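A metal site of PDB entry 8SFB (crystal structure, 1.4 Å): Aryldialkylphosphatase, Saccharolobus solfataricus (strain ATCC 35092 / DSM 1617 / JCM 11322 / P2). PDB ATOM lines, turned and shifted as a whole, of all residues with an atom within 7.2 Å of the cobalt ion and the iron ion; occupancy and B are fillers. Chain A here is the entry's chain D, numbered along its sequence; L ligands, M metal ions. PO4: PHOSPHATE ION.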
ATOM      1  N   HIS A  22      13.804   5.195 -12.729  1.00  0.00           N
ATOM      2  CA  HIS A  22      15.134   5.402 -12.155  1.00  0.00           C
ATOM      3  C   HIS A  22      15.192   4.741 -10.782  1.00  0.00           C
ATOM      4  O   HIS A  22      14.914   5.369  -9.765  1.00  0.00           O
ATOM      5  CB  HIS A  22      15.456   6.899 -12.082  1.00  0.00           C
ATOM      6  CG  HIS A  22      16.882   7.197 -11.736  1.00  0.00           C
ATOM      7  ND1 HIS A  22      17.598   8.210 -12.340  1.00  0.00           N
ATOM      8  CD2 HIS A  22      17.728   6.628 -10.845  1.00  0.00           C
ATOM      9  CE1 HIS A  22      18.821   8.246 -11.834  1.00  0.00           C
ATOM     10  NE2 HIS A  22      18.919   7.303 -10.924  1.00  0.00           N
ATOM     11  N   GLU A  23      15.582   3.455 -10.783  1.00  0.00           N
ATOM     12  CA  GLU A  23      15.779   2.681  -9.567  1.00  0.00           C
ATOM     13  C   GLU A  23      17.046   1.859  -9.718  1.00  0.00           C
ATOM     14  O   GLU A  23      17.478   1.589 -10.840  1.00  0.00           O
ATOM     15  CB  GLU A  23      14.600   1.738  -9.278  1.00  0.00           C
ATOM     16  CG  GLU A  23      13.236   2.416  -9.337  1.00  0.00           C
ATOM     17  CD  GLU A  23      12.992   3.450  -8.245  1.00  0.00           C
ATOM     18  OE1 GLU A  23      12.021   4.213  -8.368  1.00  0.00           O
ATOM     19  OE2 GLU A  23      13.753   3.454  -7.252  1.00  0.00           O
ATOM     20  N   HIS A  24      17.638   1.446  -8.597  1.00  0.00           N
ATOM     21  CA  HIS A  24      18.863   0.662  -8.612  1.00  0.00           C
ATOM     22  C   HIS A  24      18.661  -0.623  -7.824  1.00  0.00           C
ATOM     23  O   HIS A  24      18.351  -0.579  -6.632  1.00  0.00           O
ATOM     24  CB  HIS A  24      20.017   1.461  -7.997  1.00  0.00           C
ATOM     25  CG  HIS A  24      20.342   2.724  -8.732  1.00  0.00           C
ATOM     26  ND1 HIS A  24      21.148   2.752  -9.853  1.00  0.00           N
ATOM     27  CD2 HIS A  24      20.010   3.995  -8.475  1.00  0.00           C
ATOM     28  CE1 HIS A  24      21.272   4.015 -10.260  1.00  0.00           C
ATOM     29  NE2 HIS A  24      20.574   4.790  -9.444  1.00  0.00           N
ATOM     30  N   PRO A  67      19.406   2.573 -13.966  1.00  0.00           N
ATOM     31  CA  PRO A  67      20.540   3.258 -14.571  1.00  0.00           C
ATOM     32  C   PRO A  67      21.849   3.102 -13.806  1.00  0.00           C
ATOM     33  O   PRO A  67      22.624   4.052 -13.694  1.00  0.00           O
ATOM     34  CB  PRO A  67      20.074   4.719 -14.592  1.00  0.00           C
ATOM     35  CG  PRO A  67      19.243   4.829 -13.343  1.00  0.00           C
ATOM     36  CD  PRO A  67      18.567   3.483 -13.175  1.00  0.00           C
ATOM     37  N   THR A  68      22.104   1.886 -13.286  1.00  0.00           N
ATOM     38  CA  THR A  68      23.395   1.572 -12.697  1.00  0.00           C
ATOM     39  C   THR A  68      24.378   1.331 -13.844  1.00  0.00           C
ATOM     40  O   THR A  68      24.131   0.457 -14.672  1.00  0.00           O
ATOM     41  CB  THR A  68      23.304   0.334 -11.791  1.00  0.00           C
ATOM     42  OG1 THR A  68      22.262   0.483 -10.822  1.00  0.00           O
ATOM     43  CG2 THR A  68      24.598   0.061 -11.070  1.00  0.00           C
ATOM     44  N   CYS A  72      29.135   2.775 -10.576  1.00  0.00           N
ATOM     45  CA  CYS A  72      28.167   2.363  -9.571  1.00  0.00           C
ATOM     46  C   CYS A  72      27.928   0.851  -9.601  1.00  0.00           C
ATOM     47  O   CYS A  72      26.989   0.367  -8.963  1.00  0.00           O
ATOM     48  CB  CYS A  72      26.862   3.131  -9.744  1.00  0.00           C
ATOM     49  SG  CYS A  72      27.013   4.862  -9.279  1.00  0.00           S
ATOM     50  N   ILE A  97      29.337   7.183 -14.828  1.00  0.00           N
ATOM     51  CA  ILE A  97      29.125   8.185 -13.794  1.00  0.00           C
ATOM     52  C   ILE A  97      30.480   8.656 -13.288  1.00  0.00           C
ATOM     53  O   ILE A  97      31.177   7.919 -12.592  1.00  0.00           O
ATOM     54  CB  ILE A  97      28.290   7.631 -12.620  1.00  0.00           C
ATOM     55  CG1 ILE A  97      26.974   7.010 -13.090  1.00  0.00           C
ATOM     56  CG2 ILE A  97      28.067   8.704 -11.557  1.00  0.00           C
ATOM     57  CD1 ILE A  97      26.059   7.952 -13.779  1.00  0.00           C
ATOM     58  N   PHE A  99      32.220  12.548 -11.685  1.00  0.00           N
ATOM     59  CA  PHE A  99      31.992  13.938 -11.318  1.00  0.00           C
ATOM     60  C   PHE A  99      33.180  14.834 -11.678  1.00  0.00           C
ATOM     61  O   PHE A  99      33.012  16.051 -11.782  1.00  0.00           O
ATOM     62  CB  PHE A  99      31.701  14.082  -9.819  1.00  0.00           C
ATOM     63  CG  PHE A  99      30.414  13.450  -9.362  1.00  0.00           C
ATOM     64  CD1 PHE A  99      29.492  12.958 -10.276  1.00  0.00           C
ATOM     65  CD2 PHE A  99      30.112  13.372  -8.018  1.00  0.00           C
ATOM     66  CE1 PHE A  99      28.309  12.372  -9.849  1.00  0.00           C
ATOM     67  CE2 PHE A  99      28.922  12.797  -7.585  1.00  0.00           C
ATOM     68  CZ  PHE A  99      28.020  12.292  -8.501  1.00  0.00           C
ATOM     69  N   KCX A 137      23.408   6.459 -19.639  1.00  0.00           N
ATOM     70  CA  KCX A 137      23.398   7.244 -18.382  1.00  0.00           C
ATOM     71  CB  KCX A 137      23.220   6.286 -17.208  1.00  0.00           C
ATOM     72  CG  KCX A 137      23.368   6.918 -15.833  1.00  0.00           C
ATOM     73  CD  KCX A 137      22.287   7.928 -15.563  1.00  0.00           C
ATOM     74  CE  KCX A 137      22.384   8.506 -14.167  1.00  0.00           C
ATOM     75  NZ  KCX A 137      22.269   7.485 -13.109  1.00  0.00           N
ATOM     76  C   KCX A 137      24.698   8.032 -18.263  1.00  0.00           C
ATOM     77  O   KCX A 137      25.765   7.453 -18.424  1.00  0.00           O
ATOM     78  CX  KCX A 137      22.118   7.854 -11.832  1.00  0.00           C
ATOM     79  OQ1 KCX A 137      22.053   6.879 -10.973  1.00  0.00           O
ATOM     80  OQ2 KCX A 137      22.059   9.028 -11.492  1.00  0.00           O
ATOM     81  N   ILE A 138      24.564   9.319 -17.932  1.00  0.00           N
ATOM     82  CA  ILE A 138      25.732  10.223 -17.742  1.00  0.00           C
ATOM     83  C   ILE A 138      25.474  11.088 -16.503  1.00  0.00           C
ATOM     84  O   ILE A 138      24.352  11.127 -16.017  1.00  0.00           O
ATOM     85  CB  ILE A 138      25.960  11.116 -18.978  1.00  0.00           C
ATOM     86  CG1 ILE A 138      24.758  12.034 -19.223  1.00  0.00           C
ATOM     87  CG2 ILE A 138      26.305  10.277 -20.193  1.00  0.00           C
ATOM     88  CD1 ILE A 138      24.916  12.974 -20.388  1.00  0.00           C
ATOM     89  N   ALA A 139      26.513  11.792 -16.022  1.00  0.00           N
ATOM     90  CA  ALA A 139      26.440  12.515 -14.761  1.00  0.00           C
ATOM     91  C   ALA A 139      27.223  13.817 -14.800  1.00  0.00           C
ATOM     92  O   ALA A 139      28.165  13.994 -15.568  1.00  0.00           O
ATOM     93  CB  ALA A 139      26.953  11.676 -13.611  1.00  0.00           C
ATOM     94  N   ASP A 141      27.952  16.832 -11.279  1.00  0.00           N
ATOM     95  CA  ASP A 141      27.518  17.191  -9.944  1.00  0.00           C
ATOM     96  C   ASP A 141      28.165  18.505  -9.528  1.00  0.00           C
ATOM     97  O   ASP A 141      28.290  19.428 -10.337  1.00  0.00           O
ATOM     98  CB  ASP A 141      27.810  16.052  -8.967  1.00  0.00           C
ATOM     99  CG  ASP A 141      26.875  16.039  -7.769  1.00  0.00           C
ATOM    100  OD1 ASP A 141      25.814  15.375  -7.846  1.00  0.00           O
ATOM    101  OD2 ASP A 141      27.191  16.709  -6.767  1.00  0.00           O
ATOM    102  N   THR A 169      20.166  11.381 -17.179  1.00  0.00           N
ATOM    103  CA  THR A 169      21.273  12.054 -16.520  1.00  0.00           C
ATOM    104  C   THR A 169      21.117  12.055 -15.005  1.00  0.00           C
ATOM    105  O   THR A 169      20.015  11.956 -14.458  1.00  0.00           O
ATOM    106  CB  THR A 169      21.496  13.490 -17.029  1.00  0.00           C
ATOM    107  OG1 THR A 169      20.700  14.395 -16.265  1.00  0.00           O
ATOM    108  CG2 THR A 169      21.187  13.639 -18.508  1.00  0.00           C
ATOM    109  N   HIS A 170      22.278  12.152 -14.360  1.00  0.00           N
ATOM    110  CA  HIS A 170      22.425  12.561 -12.983  1.00  0.00           C
ATOM    111  C   HIS A 170      22.883  14.013 -13.008  1.00  0.00           C
ATOM    112  O   HIS A 170      23.850  14.343 -13.686  1.00  0.00           O
ATOM    113  CB  HIS A 170      23.526  11.725 -12.339  1.00  0.00           C
ATOM    114  CG  HIS A 170      23.950  12.185 -10.999  1.00  0.00           C
ATOM    115  ND1 HIS A 170      23.658  11.480  -9.849  1.00  0.00           N
ATOM    116  CD2 HIS A 170      24.639  13.272 -10.607  1.00  0.00           C
ATOM    117  CE1 HIS A 170      24.167  12.118  -8.812  1.00  0.00           C
ATOM    118  NE2 HIS A 170      24.764  13.219  -9.239  1.00  0.00           N
ATOM    119  N   SER A 171      22.173  14.877 -12.288  1.00  0.00           N
ATOM    120  CA  SER A 171      22.609  16.262 -12.158  1.00  0.00           C
ATOM    121  C   SER A 171      22.549  16.698 -10.703  1.00  0.00           C
ATOM    122  O   SER A 171      22.007  15.988  -9.851  1.00  0.00           O
ATOM    123  CB  SER A 171      21.816  17.219 -13.057  1.00  0.00           C
ATOM    124  OG  SER A 171      20.581  17.614 -12.475  1.00  0.00           O
ATOM    125  N   GLY A 198      18.054  14.360 -14.574  1.00  0.00           N
ATOM    126  CA  GLY A 198      17.792  13.732 -13.290  1.00  0.00           C
ATOM    127  C   GLY A 198      18.024  14.646 -12.084  1.00  0.00           C
ATOM    128  O   GLY A 198      18.784  15.617 -12.137  1.00  0.00           O
ATOM    129  N   HIS A 199      17.327  14.280 -11.009  1.00  0.00           N
ATOM    130  CA  HIS A 199      17.539  14.772  -9.657  1.00  0.00           C
ATOM    131  C   HIS A 199      17.055  16.205  -9.509  1.00  0.00           C
ATOM    132  O   HIS A 199      17.465  16.906  -8.591  1.00  0.00           O
ATOM    133  CB  HIS A 199      18.998  14.604  -9.227  1.00  0.00           C
ATOM    134  CG  HIS A 199      19.486  13.202  -9.395  1.00  0.00           C
ATOM    135  ND1 HIS A 199      18.657  12.102  -9.393  1.00  0.00           N
ATOM    136  CD2 HIS A 199      20.742  12.737  -9.557  1.00  0.00           C
ATOM    137  CE1 HIS A 199      19.392  11.009  -9.579  1.00  0.00           C
ATOM    138  NE2 HIS A 199      20.653  11.370  -9.676  1.00  0.00           N
ATOM    139  N   ASP A 222      12.855  12.385  -9.327  1.00  0.00           N
ATOM    140  CA  ASP A 222      13.193  11.077  -8.846  1.00  0.00           C
ATOM    141  C   ASP A 222      13.240  11.189  -7.326  1.00  0.00           C
ATOM    142  O   ASP A 222      12.160  11.291  -6.646  1.00  0.00           O
ATOM    143  CB  ASP A 222      14.463  10.551  -9.538  1.00  0.00           C
ATOM    144  CG  ASP A 222      15.449  11.651  -9.924  1.00  0.00           C
ATOM    145  OD1 ASP A 222      15.975  12.285  -9.014  1.00  0.00           O
ATOM    146  OD2 ASP A 222      15.690  11.862 -11.142  1.00  0.00           O
ATOM    147  N   ARG A 223      14.469  11.324  -6.809  1.00  0.00           N
ATOM    148  CA  ARG A 223      14.866  10.818  -5.506  1.00  0.00           C
ATOM    149  C   ARG A 223      13.766  10.859  -4.437  1.00  0.00           C
ATOM    150  O   ARG A 223      14.049  11.262  -3.303  1.00  0.00           O
ATOM    151  CB  ARG A 223      16.109  11.574  -5.066  1.00  0.00           C
ATOM    152  CG  ARG A 223      17.195  11.505  -6.131  1.00  0.00           C
ATOM    153  CD  ARG A 223      18.406  12.344  -5.800  1.00  0.00           C
ATOM    154  NE  ARG A 223      19.603  11.616  -6.165  1.00  0.00           N
ATOM    155  CZ  ARG A 223      20.814  12.152  -6.184  1.00  0.00           C
ATOM    156  NH1 ARG A 223      20.950  13.445  -5.952  1.00  0.00           N
ATOM    157  NH2 ARG A 223      21.871  11.400  -6.447  1.00  0.00           N
ATOM    158  N   ASP A 256      14.804   6.523  -7.029  1.00  0.00           N
ATOM    159  CA  ASP A 256      16.256   6.407  -7.088  1.00  0.00           C
ATOM    160  C   ASP A 256      16.687   5.530  -5.930  1.00  0.00           C
ATOM    161  O   ASP A 256      17.773   5.695  -5.383  1.00  0.00           O
ATOM    162  CB  ASP A 256      16.908   7.772  -7.006  1.00  0.00           C
ATOM    163  CG  ASP A 256      18.331   7.851  -7.521  1.00  0.00           C
ATOM    164  OD1 ASP A 256      18.832   6.832  -8.014  1.00  0.00           O
ATOM    165  OD2 ASP A 256      18.927   8.919  -7.416  1.00  0.00           O
ATOM    166  N   TYR A 257      15.800   4.608  -5.552  1.00  0.00           N
ATOM    167  CA  TYR A 257      16.052   3.759  -4.403  1.00  0.00           C
ATOM    168  C   TYR A 257      17.125   2.747  -4.784  1.00  0.00           C
ATOM    169  O   TYR A 257      17.100   2.190  -5.870  1.00  0.00           O
ATOM    170  CB  TYR A 257      14.775   3.044  -3.952  1.00  0.00           C
ATOM    171  CG  TYR A 257      14.963   2.248  -2.687  1.00  0.00           C
ATOM    172  CD1 TYR A 257      15.219   2.895  -1.489  1.00  0.00           C
ATOM    173  CD2 TYR A 257      14.939   0.863  -2.695  1.00  0.00           C
ATOM    174  CE1 TYR A 257      15.416   2.184  -0.322  1.00  0.00           C
ATOM    175  CE2 TYR A 257      15.129   0.134  -1.538  1.00  0.00           C
ATOM    176  CZ  TYR A 257      15.359   0.796  -0.346  1.00  0.00           C
ATOM    177  OH  TYR A 257      15.551   0.087   0.812  1.00  0.00           O
ATOM    178  N   TRP A 263      27.669   3.094   0.148  1.00  0.00           N
ATOM    179  CA  TRP A 263      28.043   4.392   0.698  1.00  0.00           C
ATOM    180  C   TRP A 263      27.945   4.353   2.220  1.00  0.00           C
ATOM    181  O   TRP A 263      27.004   3.773   2.775  1.00  0.00           O
ATOM    182  CB  TRP A 263      27.153   5.505   0.135  1.00  0.00           C
ATOM    183  CG  TRP A 263      27.195   5.642  -1.363  1.00  0.00           C
ATOM    184  CD1 TRP A 263      27.985   4.937  -2.234  1.00  0.00           C
ATOM    185  CD2 TRP A 263      26.418   6.539  -2.164  1.00  0.00           C
ATOM    186  NE1 TRP A 263      27.752   5.346  -3.519  1.00  0.00           N
ATOM    187  CE2 TRP A 263      26.792   6.333  -3.511  1.00  0.00           C
ATOM    188  CE3 TRP A 263      25.445   7.511  -1.881  1.00  0.00           C
ATOM    189  CZ2 TRP A 263      26.227   7.042  -4.568  1.00  0.00           C
ATOM    190  CZ3 TRP A 263      24.885   8.219  -2.930  1.00  0.00           C
ATOM    191  CH2 TRP A 263      25.276   7.988  -4.244  1.00  0.00           C
HETATM  192  P   PO4 L   1      22.045   8.288  -8.175  1.00  0.00           P
HETATM  193  O1  PO4 L   1      21.674   8.620  -6.729  1.00  0.00           O
HETATM  194  O2  PO4 L   1      20.931   8.748  -9.102  1.00  0.00           O
HETATM  195  O3  PO4 L   1      22.219   6.780  -8.317  1.00  0.00           O
HETATM  196  O4  PO4 L   1      23.341   9.005  -8.555  1.00  0.00           O
HETATM  197 CO    CO M   1      22.223   9.983  -9.646  1.00  0.00          CO
HETATM  198 FE    FE M   2      20.520   6.868  -9.484  1.00  0.00          FE
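ND1 of His 24 sits at hydrogen-bond distance from OG1 of Thr 68 (2.7 Å). The backbone NH of His 24 is in hydrogen-bond range of the backbone carbonyl oxygen of Tyr 257. A ring nitrogen (NE2) of His 170 is in hydrogen-bond range of the side-chain carboxylate (OD1) of Asp 141 (2.8 Å). The backbone NH of His 170 sits at hydrogen-bond distance from the backbone carbonyl oxygen of Ile 138 (2.8 Å). A ring nitrogen (ND1) of His 199 sits at hydrogen-bond distance from the guanidinium group (NE) of Arg 223, at 3.4 Å. A ring nitrogen (ND1) of His 199 lies within hydrogen-bond range of the side-chain carboxylate of Asp 222 (2.7 Å). The guanidinium group of Arg 223 lies within salt-bridge range of the side-chain carboxylate of Asp 256 (3.0 Å). The backbone NH (N) of Asp 256 is in hydrogen-bond range of the side-chain carboxylate (OE2) of Glu 23, at 3.3 Å.
NH2 of Arg 223 touches the cobalt ion, 3.5 Å away. Four residues have an atom within 4 Å of the cobalt ion: KCX 137, His 170, His 199 and Arg 223.
Of the 22 residues printed, 4 come within 4 Å of the iron ion. Along chain A the residues within 4 Å of the iron ion span positions 22 to 256.
The cobalt ion is bound by an oxygen (O4) of the ligand, an oxygen (O2) of the ligand, a ring nitrogen (ND1) of His 170, OQ2 of KCX 137 and a ring nitrogen (NE2) of His 199. The cobalt ion has five donor atoms within binding distance.
The iron ion is bound by O2 of the ligand (2.0 Å), O3 of the ligand (2.1 Å), NE2 of His 24 (2.1 Å), OQ1 of KCX 137 (2.1 Å), NE2 of His 22 (2.2 Å) and OD1 of Asp 256 (2.2 Å).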
